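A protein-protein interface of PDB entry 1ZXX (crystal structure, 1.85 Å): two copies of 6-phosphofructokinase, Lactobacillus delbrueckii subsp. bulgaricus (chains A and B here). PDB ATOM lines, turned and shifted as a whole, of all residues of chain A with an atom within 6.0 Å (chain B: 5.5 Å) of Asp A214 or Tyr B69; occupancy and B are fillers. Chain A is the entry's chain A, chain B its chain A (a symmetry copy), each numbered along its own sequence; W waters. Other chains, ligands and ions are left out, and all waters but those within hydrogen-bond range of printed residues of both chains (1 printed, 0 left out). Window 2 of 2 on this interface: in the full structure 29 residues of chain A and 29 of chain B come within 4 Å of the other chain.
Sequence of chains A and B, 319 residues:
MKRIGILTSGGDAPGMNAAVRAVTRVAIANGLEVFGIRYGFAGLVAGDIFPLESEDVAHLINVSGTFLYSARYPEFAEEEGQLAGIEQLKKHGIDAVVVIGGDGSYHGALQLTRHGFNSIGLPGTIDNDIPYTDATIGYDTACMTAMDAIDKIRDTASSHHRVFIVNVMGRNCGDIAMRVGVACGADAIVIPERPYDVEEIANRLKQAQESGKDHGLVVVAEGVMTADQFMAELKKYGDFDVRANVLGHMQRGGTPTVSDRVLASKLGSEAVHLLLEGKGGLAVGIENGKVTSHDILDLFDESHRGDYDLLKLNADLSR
Of the printed residues of chain B, His A160 touches Ser B70 (3.7 Å).
Printed residues of chain A within 4 Å of Tyr B39: His A161 (3.4 Å).
Of the printed residues of chain A, Thr B66 touches Ser A159 (3.0 Å).
Of chain A, only Ser A158 (3.1 Å), Ser A159 (3.4 Å), His A161 (3.4 Å) and Asp A214 (2.6 Å) come within 4 Å of Tyr B69.
Of the printed residues of chain A, Ser B70 touches Ser A159 (3.0 Å) and His A160 (3.7 Å).
The nearest printed residue of chain B that does not touch Asp A214 is Tyr B39 (6.4 Å).
The nearest residue of chain A that does not touch Tyr B69 is His A160 (4.9 Å).
The nearest printed residue of chain B that does not touch Ser A158 is Thr B66 (5.4 Å).
Of the 11 printed residues of chain B, 4 touch a printed residue of chain A.
Hydrophobic or aromatic side chains of chain B within 4 Å of the printed part of chain A: Tyr B39 and Tyr B69.
Among the printed residues, no Asp or Glu carboxylate lies within 4 Å of a Lys or Arg side-chain nitrogen of the other chain.
Water W1 lies within hydrogen-bond range of ND1 of His A161, O of Ser A159 and O of Ser B70.
No position is printed for both chains.
The side-chain hydroxyl (OG1) of Thr B8 lies within hydrogen-bond range of the backbone carbonyl oxygen (O) of Tyr B69 (3.0 Å).
The backbone NH (N) of Tyr B39 sits at hydrogen-bond distance from the backbone carbonyl oxygen (O) of Leu B68 (3.0 Å).
OG1 of Thr B66 lies within hydrogen-bond range of OG1 of Thr B8, 2.7 Å away.
The backbone NH of Tyr B39 is in hydrogen-bond range of the backbone carbonyl oxygen of Tyr B69.
The backbone NH (N) of Tyr B69 lies within hydrogen-bond range of the side-chain hydroxyl (OG1) of Thr B66 (3.4 Å).
OG of Ser A158 lies within hydrogen-bond range of OD2 of Asp A214, 3.3 Å away.
Among the printed residues, pairs that only touch across the chains: Ser A158 with Tyr B69, Ser A159 with Tyr B69, His A160 with Ser B70, His A161 with Tyr B39 and His A161 with Tyr B69.
OH of Tyr B69 is in hydrogen-bond range of OD1 of Asp A214 (2.6 Å).
OG of Ser A159 sits at hydrogen-bond distance from N of Thr B66 (3.0 Å).
The backbone NH of Ser B70 lies within hydrogen-bond range of the backbone carbonyl oxygen of Ser A159, at 3.0 Å.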
ATOM      1  N   ALA A 157      28.019  -1.928  23.863  1.00  0.00           N
ATOM      2  CA  ALA A 157      28.412  -3.072  23.042  1.00  0.00           C
ATOM      3  C   ALA A 157      27.645  -3.114  21.713  1.00  0.00           C
ATOM      4  O   ALA A 157      28.224  -3.359  20.651  1.00  0.00           O
ATOM      5  CB  ALA A 157      28.194  -4.355  23.815  1.00  0.00           C
ATOM      6  N   SER A 158      26.333  -2.867  21.771  1.00  0.00           N
ATOM      7  CA  SER A 158      25.485  -2.958  20.589  1.00  0.00           C
ATOM      8  C   SER A 158      25.753  -1.857  19.558  1.00  0.00           C
ATOM      9  O   SER A 158      25.699  -2.108  18.351  1.00  0.00           O
ATOM     10  CB  SER A 158      23.995  -2.989  20.979  1.00  0.00           C
ATOM     11  OG  SER A 158      23.729  -4.064  21.872  1.00  0.00           O
ATOM     12  N   SER A 159      26.041  -0.648  20.020  1.00  0.00           N
ATOM     13  CA  SER A 159      26.358   0.434  19.111  1.00  0.00           C
ATOM     14  C   SER A 159      27.596   0.098  18.262  1.00  0.00           C
ATOM     15  O   SER A 159      27.705   0.548  17.123  1.00  0.00           O
ATOM     16  CB  SER A 159      26.589   1.742  19.853  1.00  0.00           C
ATOM     17  OG  SER A 159      25.463   2.125  20.644  1.00  0.00           O
ATOM     18  N   HIS A 160      28.482  -0.726  18.816  1.00  0.00           N
ATOM     19  CA  HIS A 160      29.823  -0.945  18.246  1.00  0.00           C
ATOM     20  C   HIS A 160      30.091  -2.386  17.790  1.00  0.00           C
ATOM     21  O   HIS A 160      31.229  -2.723  17.395  1.00  0.00           O
ATOM     22  CB  HIS A 160      30.871  -0.508  19.260  1.00  0.00           C
ATOM     23  CG  HIS A 160      30.931   0.972  19.463  1.00  0.00           C
ATOM     24  ND1 HIS A 160      31.579   1.816  18.585  1.00  0.00           N
ATOM     25  CD2 HIS A 160      30.410   1.764  20.430  1.00  0.00           C
ATOM     26  CE1 HIS A 160      31.459   3.064  19.005  1.00  0.00           C
ATOM     27  NE2 HIS A 160      30.753   3.060  20.122  1.00  0.00           N
ATOM     28  N   HIS A 161      29.065  -3.236  17.831  1.00  0.00           N
ATOM     29  CA  HIS A 161      29.235  -4.676  17.560  1.00  0.00           C
ATOM     30  C   HIS A 161      30.426  -5.252  18.345  1.00  0.00           C
ATOM     31  O   HIS A 161      31.303  -5.908  17.776  1.00  0.00           O
ATOM     32  CB  HIS A 161      29.377  -4.933  16.049  1.00  0.00           C
ATOM     33  CG  HIS A 161      28.106  -4.739  15.274  1.00  0.00           C
ATOM     34  ND1 HIS A 161      27.526  -3.501  15.079  1.00  0.00           N
ATOM     35  CD2 HIS A 161      27.318  -5.628  14.624  1.00  0.00           C
ATOM     36  CE1 HIS A 161      26.429  -3.637  14.354  1.00  0.00           C
ATOM     37  NE2 HIS A 161      26.279  -4.919  14.064  1.00  0.00           N
ATOM     38  N   ARG A 162      30.432  -5.005  19.654  1.00  0.00           N
ATOM     39  CA  ARG A 162      31.520  -5.376  20.560  1.00  0.00           C
ATOM     40  C   ARG A 162      31.115  -6.591  21.397  1.00  0.00           C
ATOM     41  O   ARG A 162      29.929  -6.785  21.703  1.00  0.00           O
ATOM     42  CB  ARG A 162      31.799  -4.209  21.512  1.00  0.00           C
ATOM     43  CG  ARG A 162      33.189  -4.139  22.102  1.00  0.00           C
ATOM     44  CD  ARG A 162      34.183  -3.448  21.175  1.00  0.00           C
ATOM     45  NE  ARG A 162      34.100  -1.987  21.192  1.00  0.00           N
ATOM     46  CZ  ARG A 162      34.402  -1.207  20.152  1.00  0.00           C
ATOM     47  NH1 ARG A 162      34.772  -1.738  18.993  1.00  0.00           N
ATOM     48  NH2 ARG A 162      34.320   0.106  20.259  1.00  0.00           N
ATOM     49  N   ALA A 208      26.796 -16.350  16.368  1.00  0.00           N
ATOM     50  CA  ALA A 208      26.003 -15.134  16.620  1.00  0.00           C
ATOM     51  C   ALA A 208      26.416 -13.995  15.682  1.00  0.00           C
ATOM     52  O   ALA A 208      25.577 -13.347  15.058  1.00  0.00           O
ATOM     53  CB  ALA A 208      26.149 -14.704  18.086  1.00  0.00           C
ATOM     54  N   GLY A 212      24.167 -12.012  12.581  1.00  0.00           N
ATOM     55  CA  GLY A 212      23.871 -10.581  12.579  1.00  0.00           C
ATOM     56  C   GLY A 212      23.706  -9.917  13.936  1.00  0.00           C
ATOM     57  O   GLY A 212      23.295  -8.757  14.005  1.00  0.00           O
ATOM     58  N   LYS A 213      24.019 -10.645  15.006  1.00  0.00           N
ATOM     59  CA  LYS A 213      23.890 -10.132  16.369  1.00  0.00           C
ATOM     60  C   LYS A 213      24.855  -8.970  16.539  1.00  0.00           C
ATOM     61  O   LYS A 213      25.979  -9.033  16.046  1.00  0.00           O
ATOM     62  CB  LYS A 213      24.189 -11.240  17.382  1.00  0.00           C
ATOM     63  CG  LYS A 213      23.820 -10.911  18.828  1.00  0.00           C
ATOM     64  CD  LYS A 213      23.812 -12.181  19.665  1.00  0.00           C
ATOM     65  CE  LYS A 213      23.490 -11.891  21.143  1.00  0.00           C
ATOM     66  NZ  LYS A 213      23.340 -13.172  21.896  1.00  0.00           N
ATOM     67  N   ASP A 214      24.414  -7.902  17.208  1.00  0.00           N
ATOM     68  CA  ASP A 214      25.235  -6.686  17.281  1.00  0.00           C
ATOM     69  C   ASP A 214      25.954  -6.493  18.620  1.00  0.00           C
ATOM     70  O   ASP A 214      26.447  -5.412  18.911  1.00  0.00           O
ATOM     71  CB  ASP A 214      24.419  -5.441  16.900  1.00  0.00           C
ATOM     72  CG  ASP A 214      23.300  -5.151  17.880  1.00  0.00           C
ATOM     73  OD1 ASP A 214      22.421  -4.317  17.540  1.00  0.00           O
ATOM     74  OD2 ASP A 214      23.217  -5.702  19.005  1.00  0.00           O
ATOM     75  N   HIS A 215      26.034  -7.548  19.420  1.00  0.00           N
ATOM     76  CA  HIS A 215      26.701  -7.481  20.714  1.00  0.00           C
ATOM     77  C   HIS A 215      27.014  -8.874  21.195  1.00  0.00           C
ATOM     78  O   HIS A 215      26.348  -9.825  20.818  1.00  0.00           O
ATOM     79  CB  HIS A 215      25.798  -6.805  21.761  1.00  0.00           C
ATOM     80  CG  HIS A 215      24.493  -7.511  21.956  1.00  0.00           C
ATOM     81  ND1 HIS A 215      23.463  -7.426  21.043  1.00  0.00           N
ATOM     82  CD2 HIS A 215      24.068  -8.351  22.929  1.00  0.00           C
ATOM     83  CE1 HIS A 215      22.451  -8.169  21.454  1.00  0.00           C
ATOM     84  NE2 HIS A 215      22.786  -8.733  22.602  1.00  0.00           N
ATOM     85  N   GLY A 216      28.019  -8.975  22.058  1.00  0.00           N
ATOM     86  CA  GLY A 216      28.343 -10.217  22.737  1.00  0.00           C
ATOM     87  C   GLY A 216      28.588  -9.975  24.210  1.00  0.00           C
ATOM     88  O   GLY A 216      29.019  -8.890  24.620  1.00  0.00           O
ATOM     89  N   THR B   8      26.260   8.788  13.196  1.00  0.00           N
ATOM     90  CA  THR B   8      26.891   8.842  14.514  1.00  0.00           C
ATOM     91  C   THR B   8      28.268   8.226  14.404  1.00  0.00           C
ATOM     92  O   THR B   8      28.416   7.148  13.840  1.00  0.00           O
ATOM     93  CB  THR B   8      26.078   8.067  15.581  1.00  0.00           C
ATOM     94  OG1 THR B   8      25.792   6.743  15.099  1.00  0.00           O
ATOM     95  CG2 THR B   8      24.716   8.709  15.769  1.00  0.00           C
ATOM     96  N   ILE B  37      22.521   7.196   7.914  1.00  0.00           N
ATOM     97  CA  ILE B  37      23.798   6.646   7.461  1.00  0.00           C
ATOM     98  C   ILE B  37      24.349   5.810   8.611  1.00  0.00           C
ATOM     99  O   ILE B  37      24.628   6.337   9.695  1.00  0.00           O
ATOM    100  CB  ILE B  37      24.790   7.779   7.094  1.00  0.00           C
ATOM    101  CG1 ILE B  37      24.234   8.637   5.942  1.00  0.00           C
ATOM    102  CG2 ILE B  37      26.175   7.200   6.759  1.00  0.00           C
ATOM    103  CD1 ILE B  37      24.775  10.077   5.913  1.00  0.00           C
ATOM    104  N   ARG B  38      24.495   4.508   8.368  1.00  0.00           N
ATOM    105  CA  ARG B  38      24.897   3.569   9.416  1.00  0.00           C
ATOM    106  C   ARG B  38      26.422   3.516   9.578  1.00  0.00           C
ATOM    107  O   ARG B  38      27.159   3.922   8.668  1.00  0.00           O
ATOM    108  CB  ARG B  38      24.326   2.174   9.132  1.00  0.00           C
ATOM    109  CG  ARG B  38      22.793   2.088   9.160  1.00  0.00           C
ATOM    110  CD  ARG B  38      22.262   0.664   9.153  1.00  0.00           C
ATOM    111  NE  ARG B  38      20.793   0.596   9.162  1.00  0.00           N
ATOM    112  CZ  ARG B  38      20.046   0.392   8.086  1.00  0.00           C
ATOM    113  NH1 ARG B  38      18.721   0.336   8.196  1.00  0.00           N
ATOM    114  NH2 ARG B  38      20.615   0.235   6.892  1.00  0.00           N
ATOM    115  N   TYR B  39      26.875   3.037  10.737  1.00  0.00           N
ATOM    116  CA  TYR B  39      28.305   2.803  11.019  1.00  0.00           C
ATOM    117  C   TYR B  39      29.201   4.020  10.730  1.00  0.00           C
ATOM    118  O   TYR B  39      30.309   3.882  10.207  1.00  0.00           O
ATOM    119  CB  TYR B  39      28.799   1.562  10.265  1.00  0.00           C
ATOM    120  CG  TYR B  39      27.956   0.318  10.480  1.00  0.00           C
ATOM    121  CD1 TYR B  39      28.169  -0.509  11.584  1.00  0.00           C
ATOM    122  CD2 TYR B  39      26.943  -0.033   9.574  1.00  0.00           C
ATOM    123  CE1 TYR B  39      27.397  -1.656  11.788  1.00  0.00           C
ATOM    124  CE2 TYR B  39      26.161  -1.178   9.772  1.00  0.00           C
ATOM    125  CZ  TYR B  39      26.396  -1.981  10.883  1.00  0.00           C
ATOM    126  OH  TYR B  39      25.640  -3.115  11.097  1.00  0.00           O
ATOM    127  N   GLY B  40      28.718   5.208  11.087  1.00  0.00           N
ATOM    128  CA  GLY B  40      29.468   6.451  10.919  1.00  0.00           C
ATOM    129  C   GLY B  40      30.001   6.647   9.508  1.00  0.00           C
ATOM    130  O   GLY B  40      29.309   6.367   8.521  1.00  0.00           O
ATOM    131  N   THR B  66      23.461   4.147  19.767  1.00  0.00           N
ATOM    132  CA  THR B  66      23.002   4.686  18.512  1.00  0.00           C
ATOM    133  C   THR B  66      22.451   3.559  17.663  1.00  0.00           C
ATOM    134  O   THR B  66      23.133   2.562  17.396  1.00  0.00           O
ATOM    135  CB  THR B  66      24.112   5.474  17.776  1.00  0.00           C
ATOM    136  OG1 THR B  66      23.783   5.524  16.391  1.00  0.00           O
ATOM    137  CG2 THR B  66      25.457   4.719  17.808  1.00  0.00           C
ATOM    138  N   PHE B  67      21.205   3.722  17.235  1.00  0.00           N
ATOM    139  CA  PHE B  67      20.533   2.675  16.494  1.00  0.00           C
ATOM    140  C   PHE B  67      21.097   2.594  15.078  1.00  0.00           C
ATOM    141  O   PHE B  67      20.890   1.600  14.384  1.00  0.00           O
ATOM    142  CB  PHE B  67      19.012   2.909  16.479  1.00  0.00           C
ATOM    143  CG  PHE B  67      18.556   3.899  15.439  1.00  0.00           C
ATOM    144  CD1 PHE B  67      18.613   5.264  15.688  1.00  0.00           C
ATOM    145  CD2 PHE B  67      18.046   3.461  14.226  1.00  0.00           C
ATOM    146  CE1 PHE B  67      18.194   6.175  14.734  1.00  0.00           C
ATOM    147  CE2 PHE B  67      17.631   4.371  13.271  1.00  0.00           C
ATOM    148  CZ  PHE B  67      17.710   5.724  13.523  1.00  0.00           C
ATOM    149  N   LEU B  68      21.810   3.647  14.663  1.00  0.00           N
ATOM    150  CA  LEU B  68      22.462   3.678  13.338  1.00  0.00           C
ATOM    151  C   LEU B  68      23.815   2.956  13.362  1.00  0.00           C
ATOM    152  O   LEU B  68      24.390   2.657  12.300  1.00  0.00           O
ATOM    153  CB  LEU B  68      22.678   5.128  12.891  1.00  0.00           C
ATOM    154  CG  LEU B  68      21.435   5.975  12.587  1.00  0.00           C
ATOM    155  CD1 LEU B  68      21.811   7.444  12.381  1.00  0.00           C
ATOM    156  CD2 LEU B  68      20.708   5.397  11.376  1.00  0.00           C
ATOM    157  N   TYR B  69      24.294   2.686  14.578  1.00  0.00           N
ATOM    158  CA  TYR B  69      25.622   2.112  14.862  1.00  0.00           C
ATOM    159  C   TYR B  69      26.724   3.141  14.648  1.00  0.00           C
ATOM    160  O   TYR B  69      26.533   4.118  13.930  1.00  0.00           O
ATOM    161  CB  TYR B  69      25.907   0.851  14.038  1.00  0.00           C
ATOM    162  CG  TYR B  69      24.952  -0.290  14.311  1.00  0.00           C
ATOM    163  CD1 TYR B  69      24.856  -0.853  15.586  1.00  0.00           C
ATOM    164  CD2 TYR B  69      24.147  -0.796  13.306  1.00  0.00           C
ATOM    165  CE1 TYR B  69      23.969  -1.901  15.847  1.00  0.00           C
ATOM    166  CE2 TYR B  69      23.265  -1.838  13.551  1.00  0.00           C
ATOM    167  CZ  TYR B  69      23.187  -2.387  14.824  1.00  0.00           C
ATOM    168  OH  TYR B  69      22.310  -3.417  15.062  1.00  0.00           O
ATOM    169  N   SER B  70      27.863   2.920  15.304  1.00  0.00           N
ATOM    170  CA  SER B  70      29.070   3.717  15.075  1.00  0.00           C
ATOM    171  C   SER B  70      30.236   2.785  14.725  1.00  0.00           C
ATOM    172  O   SER B  70      30.269   1.634  15.152  1.00  0.00           O
ATOM    173  CB  SER B  70      29.386   4.550  16.316  1.00  0.00           C
ATOM    174  OG  SER B  70      30.527   5.380  16.129  1.00  0.00           O
ATOM    175  N   ALA B  71      31.182   3.275  13.931  1.00  0.00           N
ATOM    176  CA  ALA B  71      32.330   2.452  13.496  1.00  0.00           C
ATOM    177  C   ALA B  71      33.432   3.342  12.958  1.00  0.00           C
ATOM    178  O   ALA B  71      33.145   4.313  12.252  1.00  0.00           O
ATOM    179  CB  ALA B  71      31.909   1.447  12.435  1.00  0.00           C
HETATM  180  O   HOH W   1      28.854  -1.244  15.060  1.00  0.00           O
